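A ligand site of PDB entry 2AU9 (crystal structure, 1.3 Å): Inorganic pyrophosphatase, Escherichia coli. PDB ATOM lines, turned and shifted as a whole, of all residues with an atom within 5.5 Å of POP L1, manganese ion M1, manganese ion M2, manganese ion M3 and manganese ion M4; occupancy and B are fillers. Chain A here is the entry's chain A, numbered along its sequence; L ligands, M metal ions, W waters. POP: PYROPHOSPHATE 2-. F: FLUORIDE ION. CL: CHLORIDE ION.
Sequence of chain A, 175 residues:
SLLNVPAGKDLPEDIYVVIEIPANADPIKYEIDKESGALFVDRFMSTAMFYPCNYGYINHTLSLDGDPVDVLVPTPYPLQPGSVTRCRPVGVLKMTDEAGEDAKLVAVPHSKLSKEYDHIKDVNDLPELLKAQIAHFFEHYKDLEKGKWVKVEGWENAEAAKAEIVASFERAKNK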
ATOM      1  N   GLU A  20      -0.722   7.299  12.376  1.00  0.00           N
ATOM      2  CA  GLU A  20      -2.117   7.437  12.039  1.00  0.00           C
ATOM      3  C   GLU A  20      -2.812   6.163  11.680  1.00  0.00           C
ATOM      4  O   GLU A  20      -4.006   5.979  11.967  1.00  0.00           O
ATOM      5  CB  GLU A  20      -2.273   8.378  10.807  1.00  0.00           C
ATOM      6  CG  GLU A  20      -1.854   9.803  11.165  1.00  0.00           C
ATOM      7  CD  GLU A  20      -1.616  10.688   9.949  1.00  0.00           C
ATOM      8  OE1 GLU A  20      -0.982  10.189   9.021  1.00  0.00           O
ATOM      9  OE2 GLU A  20      -2.068  11.876  10.020  1.00  0.00           O
ATOM     10  N   LYS A  29      -8.547   5.277   6.403  1.00  0.00           N
ATOM     11  CA  LYS A  29      -7.443   6.184   6.223  1.00  0.00           C
ATOM     12  C   LYS A  29      -7.585   7.347   7.202  1.00  0.00           C
ATOM     13  O   LYS A  29      -8.158   8.430   6.910  1.00  0.00           O
ATOM     14  CB  LYS A  29      -7.364   6.687   4.759  1.00  0.00           C
ATOM     15  CG  LYS A  29      -5.952   6.988   4.321  1.00  0.00           C
ATOM     16  CD  LYS A  29      -5.256   8.201   4.826  1.00  0.00           C
ATOM     17  CE  LYS A  29      -3.873   8.508   4.265  1.00  0.00           C
ATOM     18  NZ  LYS A  29      -3.193   9.645   4.866  1.00  0.00           N
ATOM     19  N   GLU A  31      -6.320  10.561   9.408  1.00  0.00           N
ATOM     20  CA  GLU A  31      -5.343  11.659   9.358  1.00  0.00           C
ATOM     21  C   GLU A  31      -5.526  12.509  10.582  1.00  0.00           C
ATOM     22  O   GLU A  31      -6.667  12.906  10.896  1.00  0.00           O
ATOM     23  CB  GLU A  31      -5.448  12.495   8.102  1.00  0.00           C
ATOM     24  CG  GLU A  31      -5.128  11.707   6.891  1.00  0.00           C
ATOM     25  CD  GLU A  31      -5.111  12.507   5.592  1.00  0.00           C
ATOM     26  OE1 GLU A  31      -5.406  13.689   5.576  1.00  0.00           O
ATOM     27  OE2 GLU A  31      -4.776  11.973   4.517  1.00  0.00           O
ATOM     28  N   ASP A  42     -10.106  10.408   7.062  1.00  0.00           N
ATOM     29  CA  ASP A  42      -9.970  11.112   5.792  1.00  0.00           C
ATOM     30  C   ASP A  42     -10.912  10.465   4.784  1.00  0.00           C
ATOM     31  O   ASP A  42     -11.683  11.128   4.022  1.00  0.00           O
ATOM     32  CB  ASP A  42      -8.523  11.190   5.313  1.00  0.00           C
ATOM     33  CG  ASP A  42      -8.472  11.829   3.939  1.00  0.00           C
ATOM     34  OD1 ASP A  42      -8.520  13.079   3.860  1.00  0.00           O
ATOM     35  OD2 ASP A  42      -8.389  11.182   2.899  1.00  0.00           O
ATOM     36  N   ARG A  43     -10.904   9.118   4.741  1.00  0.00           N
ATOM     37  CA  ARG A  43     -11.695   8.298   3.835  1.00  0.00           C
ATOM     38  C   ARG A  43     -11.597   6.830   4.190  1.00  0.00           C
ATOM     39  O   ARG A  43     -10.703   6.436   4.941  1.00  0.00           O
ATOM     40  CB  ARG A  43     -11.312   8.475   2.346  1.00  0.00           C
ATOM     41  CG  ARG A  43      -9.941   7.913   2.030  1.00  0.00           C
ATOM     42  CD  ARG A  43      -9.477   8.429   0.639  1.00  0.00           C
ATOM     43  NE  ARG A  43      -8.196   7.887   0.214  1.00  0.00           N
ATOM     44  CZ  ARG A  43      -6.962   8.290   0.522  1.00  0.00           C
ATOM     45  NH1 ARG A  43      -6.785   9.321   1.366  1.00  0.00           N
ATOM     46  NH2 ARG A  43      -5.868   7.704   0.040  1.00  0.00           N
ATOM     47  N   TYR A  51      -1.780  -1.105   4.539  1.00  0.00           N
ATOM     48  CA  TYR A  51      -0.438  -0.511   4.631  1.00  0.00           C
ATOM     49  C   TYR A  51       0.542  -1.562   5.103  1.00  0.00           C
ATOM     50  O   TYR A  51       0.274  -2.277   6.096  1.00  0.00           O
ATOM     51  CB  TYR A  51      -0.394   0.663   5.593  1.00  0.00           C
ATOM     52  CG  TYR A  51      -0.967   1.910   5.009  1.00  0.00           C
ATOM     53  CD1 TYR A  51      -2.356   2.133   4.967  1.00  0.00           C
ATOM     54  CD2 TYR A  51      -0.198   2.907   4.431  1.00  0.00           C
ATOM     55  CE1 TYR A  51      -2.909   3.289   4.401  1.00  0.00           C
ATOM     56  CE2 TYR A  51      -0.709   4.054   3.876  1.00  0.00           C
ATOM     57  CZ  TYR A  51      -2.065   4.232   3.872  1.00  0.00           C
ATOM     58  OH  TYR A  51      -2.644   5.333   3.328  1.00  0.00           O
ATOM     59  N   TYR A  55       1.890   3.675   9.510  1.00  0.00           N
ATOM     60  CA  TYR A  55       1.979   4.860   8.682  1.00  0.00           C
ATOM     61  C   TYR A  55       1.606   6.105   9.471  1.00  0.00           C
ATOM     62  O   TYR A  55       0.627   6.132  10.184  1.00  0.00           O
ATOM     63  CB  TYR A  55       1.023   4.738   7.519  1.00  0.00           C
ATOM     64  CG  TYR A  55       1.055   5.840   6.486  1.00  0.00           C
ATOM     65  CD1 TYR A  55       2.071   5.887   5.557  1.00  0.00           C
ATOM     66  CD2 TYR A  55       0.082   6.825   6.481  1.00  0.00           C
ATOM     67  CE1 TYR A  55       2.121   6.893   4.638  1.00  0.00           C
ATOM     68  CE2 TYR A  55       0.118   7.854   5.523  1.00  0.00           C
ATOM     69  CZ  TYR A  55       1.138   7.866   4.607  1.00  0.00           C
ATOM     70  OH  TYR A  55       1.195   8.843   3.635  1.00  0.00           O
ATOM     71  N   GLY A  56       2.430   7.168   9.313  1.00  0.00           N
ATOM     72  CA  GLY A  56       2.132   8.423   9.911  1.00  0.00           C
ATOM     73  C   GLY A  56       3.027   9.556   9.389  1.00  0.00           C
ATOM     74  O   GLY A  56       3.222   9.620   8.175  1.00  0.00           O
ATOM     75  N   TYR A  57       3.468  10.412  10.331  1.00  0.00           N
ATOM     76  CA  TYR A  57       4.183  11.616   9.900  1.00  0.00           C
ATOM     77  C   TYR A  57       5.133  12.112  10.961  1.00  0.00           C
ATOM     78  O   TYR A  57       4.997  11.679  12.079  1.00  0.00           O
ATOM     79  CB  TYR A  57       3.149  12.675   9.461  1.00  0.00           C
ATOM     80  CG  TYR A  57       2.357  13.211  10.633  1.00  0.00           C
ATOM     81  CD1 TYR A  57       1.213  12.518  11.042  1.00  0.00           C
ATOM     82  CD2 TYR A  57       2.678  14.315  11.375  1.00  0.00           C
ATOM     83  CE1 TYR A  57       0.454  12.974  12.109  1.00  0.00           C
ATOM     84  CE2 TYR A  57       1.928  14.778  12.451  1.00  0.00           C
ATOM     85  CZ  TYR A  57       0.803  14.082  12.822  1.00  0.00           C
ATOM     86  OH  TYR A  57       0.041  14.462  13.861  1.00  0.00           O
ATOM     87  N   SER A  63       5.543  18.749   3.652  1.00  0.00           N
ATOM     88  CA  SER A  63       5.768  18.272   2.302  1.00  0.00           C
ATOM     89  C   SER A  63       5.118  19.235   1.341  1.00  0.00           C
ATOM     90  O   SER A  63       4.402  20.118   1.739  1.00  0.00           O
ATOM     91  CB  SER A  63       5.080  16.917   2.199  1.00  0.00           C
ATOM     92  OG  SER A  63       5.641  16.035   1.255  1.00  0.00           O
ATOM     93  N   ASP A  65       2.864  18.337  -0.576  1.00  0.00           N
ATOM     94  CA  ASP A  65       1.435  18.007  -0.711  1.00  0.00           C
ATOM     95  C   ASP A  65       0.593  18.738   0.347  1.00  0.00           C
ATOM     96  O   ASP A  65      -0.612  18.487   0.462  1.00  0.00           O
ATOM     97  CB  ASP A  65       1.199  16.516  -0.646  1.00  0.00           C
ATOM     98  CG  ASP A  65       1.332  15.922   0.742  1.00  0.00           C
ATOM     99  OD1 ASP A  65       0.821  14.811   0.965  1.00  0.00           O
ATOM    100  OD2 ASP A  65       2.005  16.561   1.565  1.00  0.00           O
ATOM    101  N   ASP A  67       0.992  18.618   3.626  1.00  0.00           N
ATOM    102  CA  ASP A  67       0.883  17.858   4.858  1.00  0.00           C
ATOM    103  C   ASP A  67       2.268  17.626   5.433  1.00  0.00           C
ATOM    104  O   ASP A  67       3.240  17.625   4.661  1.00  0.00           O
ATOM    105  CB  ASP A  67       0.222  16.506   4.615  1.00  0.00           C
ATOM    106  CG  ASP A  67      -1.152  16.326   4.058  1.00  0.00           C
ATOM    107  OD1 ASP A  67      -1.904  17.318   4.150  1.00  0.00           O
ATOM    108  OD2 ASP A  67      -1.528  15.194   3.522  1.00  0.00           O
ATOM    109  N   PRO A  68       2.416  17.337   6.728  1.00  0.00           N
ATOM    110  CA  PRO A  68       3.734  16.848   7.242  1.00  0.00           C
ATOM    111  C   PRO A  68       4.249  15.654   6.470  1.00  0.00           C
ATOM    112  O   PRO A  68       3.510  14.855   5.921  1.00  0.00           O
ATOM    113  CB  PRO A  68       3.412  16.484   8.693  1.00  0.00           C
ATOM    114  CG  PRO A  68       2.200  17.282   9.069  1.00  0.00           C
ATOM    115  CD  PRO A  68       1.415  17.463   7.822  1.00  0.00           C
ATOM    116  N   ASP A  70       5.538  12.133   5.318  1.00  0.00           N
ATOM    117  CA  ASP A  70       5.002  10.848   5.574  1.00  0.00           C
ATOM    118  C   ASP A  70       6.092   9.846   5.895  1.00  0.00           C
ATOM    119  O   ASP A  70       7.180   9.792   5.266  1.00  0.00           O
ATOM    120  CB  ASP A  70       4.190  10.316   4.388  1.00  0.00           C
ATOM    121  CG  ASP A  70       3.041  11.249   4.044  1.00  0.00           C
ATOM    122  OD1 ASP A  70       2.409  11.665   5.044  1.00  0.00           O
ATOM    123  OD2 ASP A  70       2.760  11.445   2.844  1.00  0.00           O
ATOM    124  N   MET A  95       8.011   9.615  -4.614  1.00  0.00           N
ATOM    125  CA  MET A  95       6.780   9.495  -5.387  1.00  0.00           C
ATOM    126  C   MET A  95       6.049  10.840  -5.374  1.00  0.00           C
ATOM    127  O   MET A  95       6.226  11.752  -4.548  1.00  0.00           O
ATOM    128  CB  MET A  95       5.781   8.453  -4.880  1.00  0.00           C
ATOM    129  CG  MET A  95       5.447   8.644  -3.386  1.00  0.00           C
ATOM    130  SD  MET A  95       3.951   7.747  -2.868  1.00  0.00           S
ATOM    131  CE  MET A  95       2.754   8.972  -3.380  1.00  0.00           C
ATOM    132  N   ASP A  97       1.934  12.484  -5.870  1.00  0.00           N
ATOM    133  CA  ASP A  97       0.543  12.116  -6.002  1.00  0.00           C
ATOM    134  C   ASP A  97      -0.231  13.388  -6.316  1.00  0.00           C
ATOM    135  O   ASP A  97       0.331  14.424  -6.628  1.00  0.00           O
ATOM    136  CB  ASP A  97      -0.011  11.293  -4.825  1.00  0.00           C
ATOM    137  CG  ASP A  97      -0.319  12.019  -3.543  1.00  0.00           C
ATOM    138  OD1 ASP A  97      -0.305  13.262  -3.398  1.00  0.00           O
ATOM    139  OD2 ASP A  97      -0.676  11.245  -2.601  1.00  0.00           O
ATOM    140  N   GLU A  98      -1.558  13.268  -6.352  1.00  0.00           N
ATOM    141  CA  GLU A  98      -2.400  14.378  -6.878  1.00  0.00           C
ATOM    142  C   GLU A  98      -2.228  15.627  -6.061  1.00  0.00           C
ATOM    143  O   GLU A  98      -2.585  16.719  -6.563  1.00  0.00           O
ATOM    144  CB  GLU A  98      -3.909  14.027  -6.898  1.00  0.00           C
ATOM    145  CG  GLU A  98      -4.582  13.830  -5.545  1.00  0.00           C
ATOM    146  CD  GLU A  98      -4.169  12.779  -4.571  1.00  0.00           C
ATOM    147  OE1 GLU A  98      -3.683  11.745  -5.070  1.00  0.00           O
ATOM    148  OE2 GLU A  98      -4.322  12.941  -3.325  1.00  0.00           O
ATOM    149  N   ASP A 102       5.446  13.836  -2.774  1.00  0.00           N
ATOM    150  CA  ASP A 102       4.939  13.231  -1.575  1.00  0.00           C
ATOM    151  C   ASP A 102       5.724  12.006  -1.174  1.00  0.00           C
ATOM    152  O   ASP A 102       5.182  10.881  -1.079  1.00  0.00           O
ATOM    153  CB  ASP A 102       3.465  12.866  -1.908  1.00  0.00           C
ATOM    154  CG  ASP A 102       2.637  12.495  -0.686  1.00  0.00           C
ATOM    155  OD1 ASP A 102       2.994  12.991   0.468  1.00  0.00           O
ATOM    156  OD2 ASP A 102       1.661  11.746  -0.804  1.00  0.00           O
ATOM    157  N   LYS A 104       7.761   9.005   0.700  1.00  0.00           N
ATOM    158  CA  LYS A 104       7.432   8.088   1.771  1.00  0.00           C
ATOM    159  C   LYS A 104       8.724   7.662   2.449  1.00  0.00           C
ATOM    160  O   LYS A 104       9.483   6.829   1.961  1.00  0.00           O
ATOM    161  CB  LYS A 104       6.628   6.900   1.225  1.00  0.00           C
ATOM    162  CG  LYS A 104       5.326   7.293   0.560  1.00  0.00           C
ATOM    163  CD  LYS A 104       4.276   7.736   1.545  1.00  0.00           C
ATOM    164  CE  LYS A 104       3.050   8.240   0.856  1.00  0.00           C
ATOM    165  NZ  LYS A 104       3.137   9.696   0.646  1.00  0.00           N
ATOM    166  N   TYR A 141      -3.071   1.620  -4.510  1.00  0.00           N
ATOM    167  CA  TYR A 141      -4.089   1.817  -3.477  1.00  0.00           C
ATOM    168  C   TYR A 141      -5.125   2.895  -3.873  1.00  0.00           C
ATOM    169  O   TYR A 141      -6.244   2.848  -3.316  1.00  0.00           O
ATOM    170  CB  TYR A 141      -3.496   2.138  -2.101  1.00  0.00           C
ATOM    171  CG  TYR A 141      -3.012   3.566  -1.861  1.00  0.00           C
ATOM    172  CD1 TYR A 141      -2.068   4.180  -2.689  1.00  0.00           C
ATOM    173  CD2 TYR A 141      -3.519   4.271  -0.755  1.00  0.00           C
ATOM    174  CE1 TYR A 141      -1.649   5.466  -2.435  1.00  0.00           C
ATOM    175  CE2 TYR A 141      -3.087   5.559  -0.515  1.00  0.00           C
ATOM    176  CZ  TYR A 141      -2.155   6.138  -1.360  1.00  0.00           C
ATOM    177  OH  TYR A 141      -1.703   7.437  -1.170  1.00  0.00           O
ATOM    178  N   LYS A 142      -4.809   3.804  -4.792  1.00  0.00           N
ATOM    179  CA  LYS A 142      -5.689   4.810  -5.301  1.00  0.00           C
ATOM    180  C   LYS A 142      -6.358   4.424  -6.635  1.00  0.00           C
ATOM    181  O   LYS A 142      -7.017   5.303  -7.245  1.00  0.00           O
ATOM    182  CB  LYS A 142      -4.977   6.194  -5.433  1.00  0.00           C
ATOM    183  CG  LYS A 142      -4.684   6.769  -4.079  1.00  0.00           C
ATOM    184  CD  LYS A 142      -3.777   7.995  -4.107  1.00  0.00           C
ATOM    185  CE  LYS A 142      -3.953   8.864  -2.914  1.00  0.00           C
ATOM    186  NZ  LYS A 142      -3.076  10.003  -2.913  1.00  0.00           N
HETATM  187  P1  POP L   1      -2.996  10.032   0.931  1.00  0.00           P
HETATM  188  O1  POP L   1      -2.391  10.879  -0.168  1.00  0.00           O
HETATM  189  O2  POP L   1      -3.246   8.561   0.738  1.00  0.00           O
HETATM  190  O3  POP L   1      -4.195  10.733   1.580  1.00  0.00           O
HETATM  191  O   POP L   1      -1.878  10.097   2.154  1.00  0.00           O
HETATM  192  P2  POP L   1      -1.065  11.429   2.702  1.00  0.00           P
HETATM  193  O4  POP L   1      -0.086  11.791   1.634  1.00  0.00           O
HETATM  194  O5  POP L   1      -0.415  10.880   3.947  1.00  0.00           O
HETATM  195  O6  POP L   1      -2.154  12.320   2.946  1.00  0.00           O
HETATM  196  F     F L   2       0.297  13.597   3.794  1.00  0.00           F
HETATM  197 CL    CL L   3       0.077   9.127  -0.516  1.00  0.00          CL
HETATM  198 MN    MN M   1       1.609  13.124   2.140  1.00  0.00          MN
HETATM  199 MN    MN M   2       0.356  12.246   5.467  1.00  0.00          MN
HETATM  200 MN    MN M   3      -0.374  11.423  -0.484  1.00  0.00          MN
HETATM  201 MN    MN M   4      -4.248  12.678   2.442  1.00  0.00          MN
HETATM  202  O   HOH W   1      -6.334  12.912   1.735  1.00  0.00           O
HETATM  203  O   HOH W   2       3.020  14.475   3.101  1.00  0.00           O
HETATM  204  O   HOH W   3       0.909  13.857   6.614  1.00  0.00           O
HETATM  205  O   HOH W   4      -0.850  13.575  -0.719  1.00  0.00           O
HETATM  206  O   HOH W   5      -0.991   7.274   2.081  1.00  0.00           O
HETATM  207  O   HOH W   6      -4.208  14.590   3.263  1.00  0.00           O
HETATM  208  O   HOH W   7      -3.617  13.633   0.433  1.00  0.00           O
HETATM  209  O   HOH W   8       0.613  10.866   7.074  1.00  0.00           O
HETATM  210  O   HOH W   9      -5.426  11.536  -1.205  1.00  0.00           O
HETATM  211  O   HOH W  10      -1.825  12.737   5.744  1.00  0.00           O
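OH of Tyr 55 lies close to O5 of POP L1 (2.6 Å).
The side-chain hydroxyl (OH) of Tyr 141 is in hydrogen-bond range of an oxygen (O2) of POP L1, 2.7 Å away.
The guanidinium group (NH2) of Arg 43 is in salt-bridge range of an oxygen (O2) of POP L1, at 2.8 Å.
The side-chain amino group of Lys 142 lies within salt-bridge range of an oxygen (O2) of POP L1 (3.9 Å).
NZ of Lys 29 lies within hydrogen-bond range of O of POP L1.
O4 of POP L1 sits close to NZ of Lys 104 (3.97 Å).
The side-chain carboxylate (OD2) of Asp 70 sits close to the side-chain hydroxyl (OH) of Tyr 55.
The side-chain amino group of Lys 104 sits close to the side-chain carboxylate of Asp 70, at 2.8 Å.
OD2 of Asp 65 sits at hydrogen-bond distance from N of Asp 67, at 3.1 Å.
The backbone NH (N) of Glu 20 sits at hydrogen-bond distance from the backbone carbonyl oxygen (O) of Tyr 55, 2.8 Å away.
NZ of Lys 142 lies close to OH of Tyr 141.
The backbone carbonyl oxygen of Arg 43 sits at hydrogen-bond distance from the backbone NH of Lys 29 (2.9 Å).
The guanidinium group (NH1) of Arg 43 lies within salt-bridge range of the side-chain carboxylate (OD2) of Asp 42 (2.9 Å).
The side-chain carboxylate (OE1) of Glu 98 lies within salt-bridge range of the side-chain amino group (NZ) of Lys 142, 2.8 Å away.
OD2 of Asp 67 lies close to O6 of POP L1 (3.0 Å).
Hydrophobic or aromatic side chains within 4 Å of POP L1: Tyr 55 and Tyr 141.
12 residues have an atom within 4 Å of POP L1: Lys 29, Glu 31, Arg 43, Tyr 55, Asp 65, Asp 67, Asp 70, Asp 97, Asp 102, Lys 104, Tyr 141 and Lys 142.
Within 4 Å of manganese ion M1: Asp 65, Asp 70 and Asp 102.
Merely in contact with manganese ion M2: Tyr 55.
Of the 21 residues printed, 2 come within 4 Å of manganese ion M2.
The nearest printed residue that does not touch manganese ion M2 is Asp 67 (4.003 Å).
NZ of Lys 142 touches manganese ion M3, 3.9 Å away.
Within 4 Å of manganese ion M3: Asp 65, Asp 97, Asp 102 and Lys 142.
Along chain A the residues within 4 Å of manganese ion M3 span positions 65 to 142.
Merely in contact with manganese ion M4: Asp 67 (3.9 Å).
Two residues have an atom within 4 Å of manganese ion M4: Glu 31 and Asp 67.
Manganese ion M1 is bound by the side-chain carboxylate of Asp 70 (2.2 Å), a fluorine (F) of F L2 (2.2 Å), the side-chain carboxylate of Asp 102 (2.2 Å), water W2 (2.2 Å), the side-chain carboxylate of Asp 65 (2.2 Å) and an oxygen (O4) of POP L1 (2.2 Å).
Water W3 binds manganese ion M2 (2.1 Å).
Water W8 binds manganese ion M2 (2.1 Å).
Manganese ion M2 is bound by F of F L2 (2.2 Å).
Manganese ion M2 is bound by the side-chain carboxylate (OD1) of Asp 70, 2.2 Å away.
An oxygen (O5) of POP L1 is bound to manganese ion M2, 2.2 Å away.
Manganese ion M2 is bound by water W10 (2.3 Å).
Manganese ion M3 is bound by the side-chain carboxylate (OD2) of Asp 102 (2.1 Å), an oxygen (O1) of POP L1 (2.1 Å), the side-chain carboxylate (OD2) of Asp 97 (2.1 Å), an oxygen (O4) of POP L1 (2.2 Å), water W4 (2.2 Å) and a chlorine (CL) of CL L3 (2.3 Å).
Manganese ion M3 has six donor atoms within binding distance.
Manganese ion M4 is bound by water W6 (2.1 Å), an oxygen (O3) of POP L1 (2.1 Å), an oxygen (O6) of POP L1 (2.2 Å), water W1 (2.2 Å), the side-chain carboxylate (OE2) of Glu 31 (2.3 Å) and water W7 (2.3 Å).
Manganese ion M4 has six donor atoms within binding distance.
Water W2 bridges OD2 of Asp 65 (2.8 Å) and O of Pro 68 (2.9 Å).
Water W10 bridges the side-chain carboxylate (OD2) of Asp 67 (3.3 Å) and the side-chain amino group (NZ) of Lys 29 (3.5 Å).
Water W8 bridges the side-chain carboxylate of Glu 20 (2.6 Å) and the backbone carbonyl oxygen of Gly 56 (3.1 Å).
Water W6 bridges OE1 of Glu 31 (2.8 Å) and OD2 of Asp 67 (2.8 Å).
Water W5 lies within hydrogen-bond range of the side-chain hydroxyl of Tyr 51 (2.8 Å), an oxygen (O2) of POP L1 (2.9 Å), the side-chain hydroxyl of Tyr 55 (3.1 Å) and the side-chain hydroxyl of Tyr 141 (3.3 Å).
Water W9 lies within hydrogen-bond range of OE2 of Glu 98 (2.8 Å) and NZ of Lys 142 (3.3 Å).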
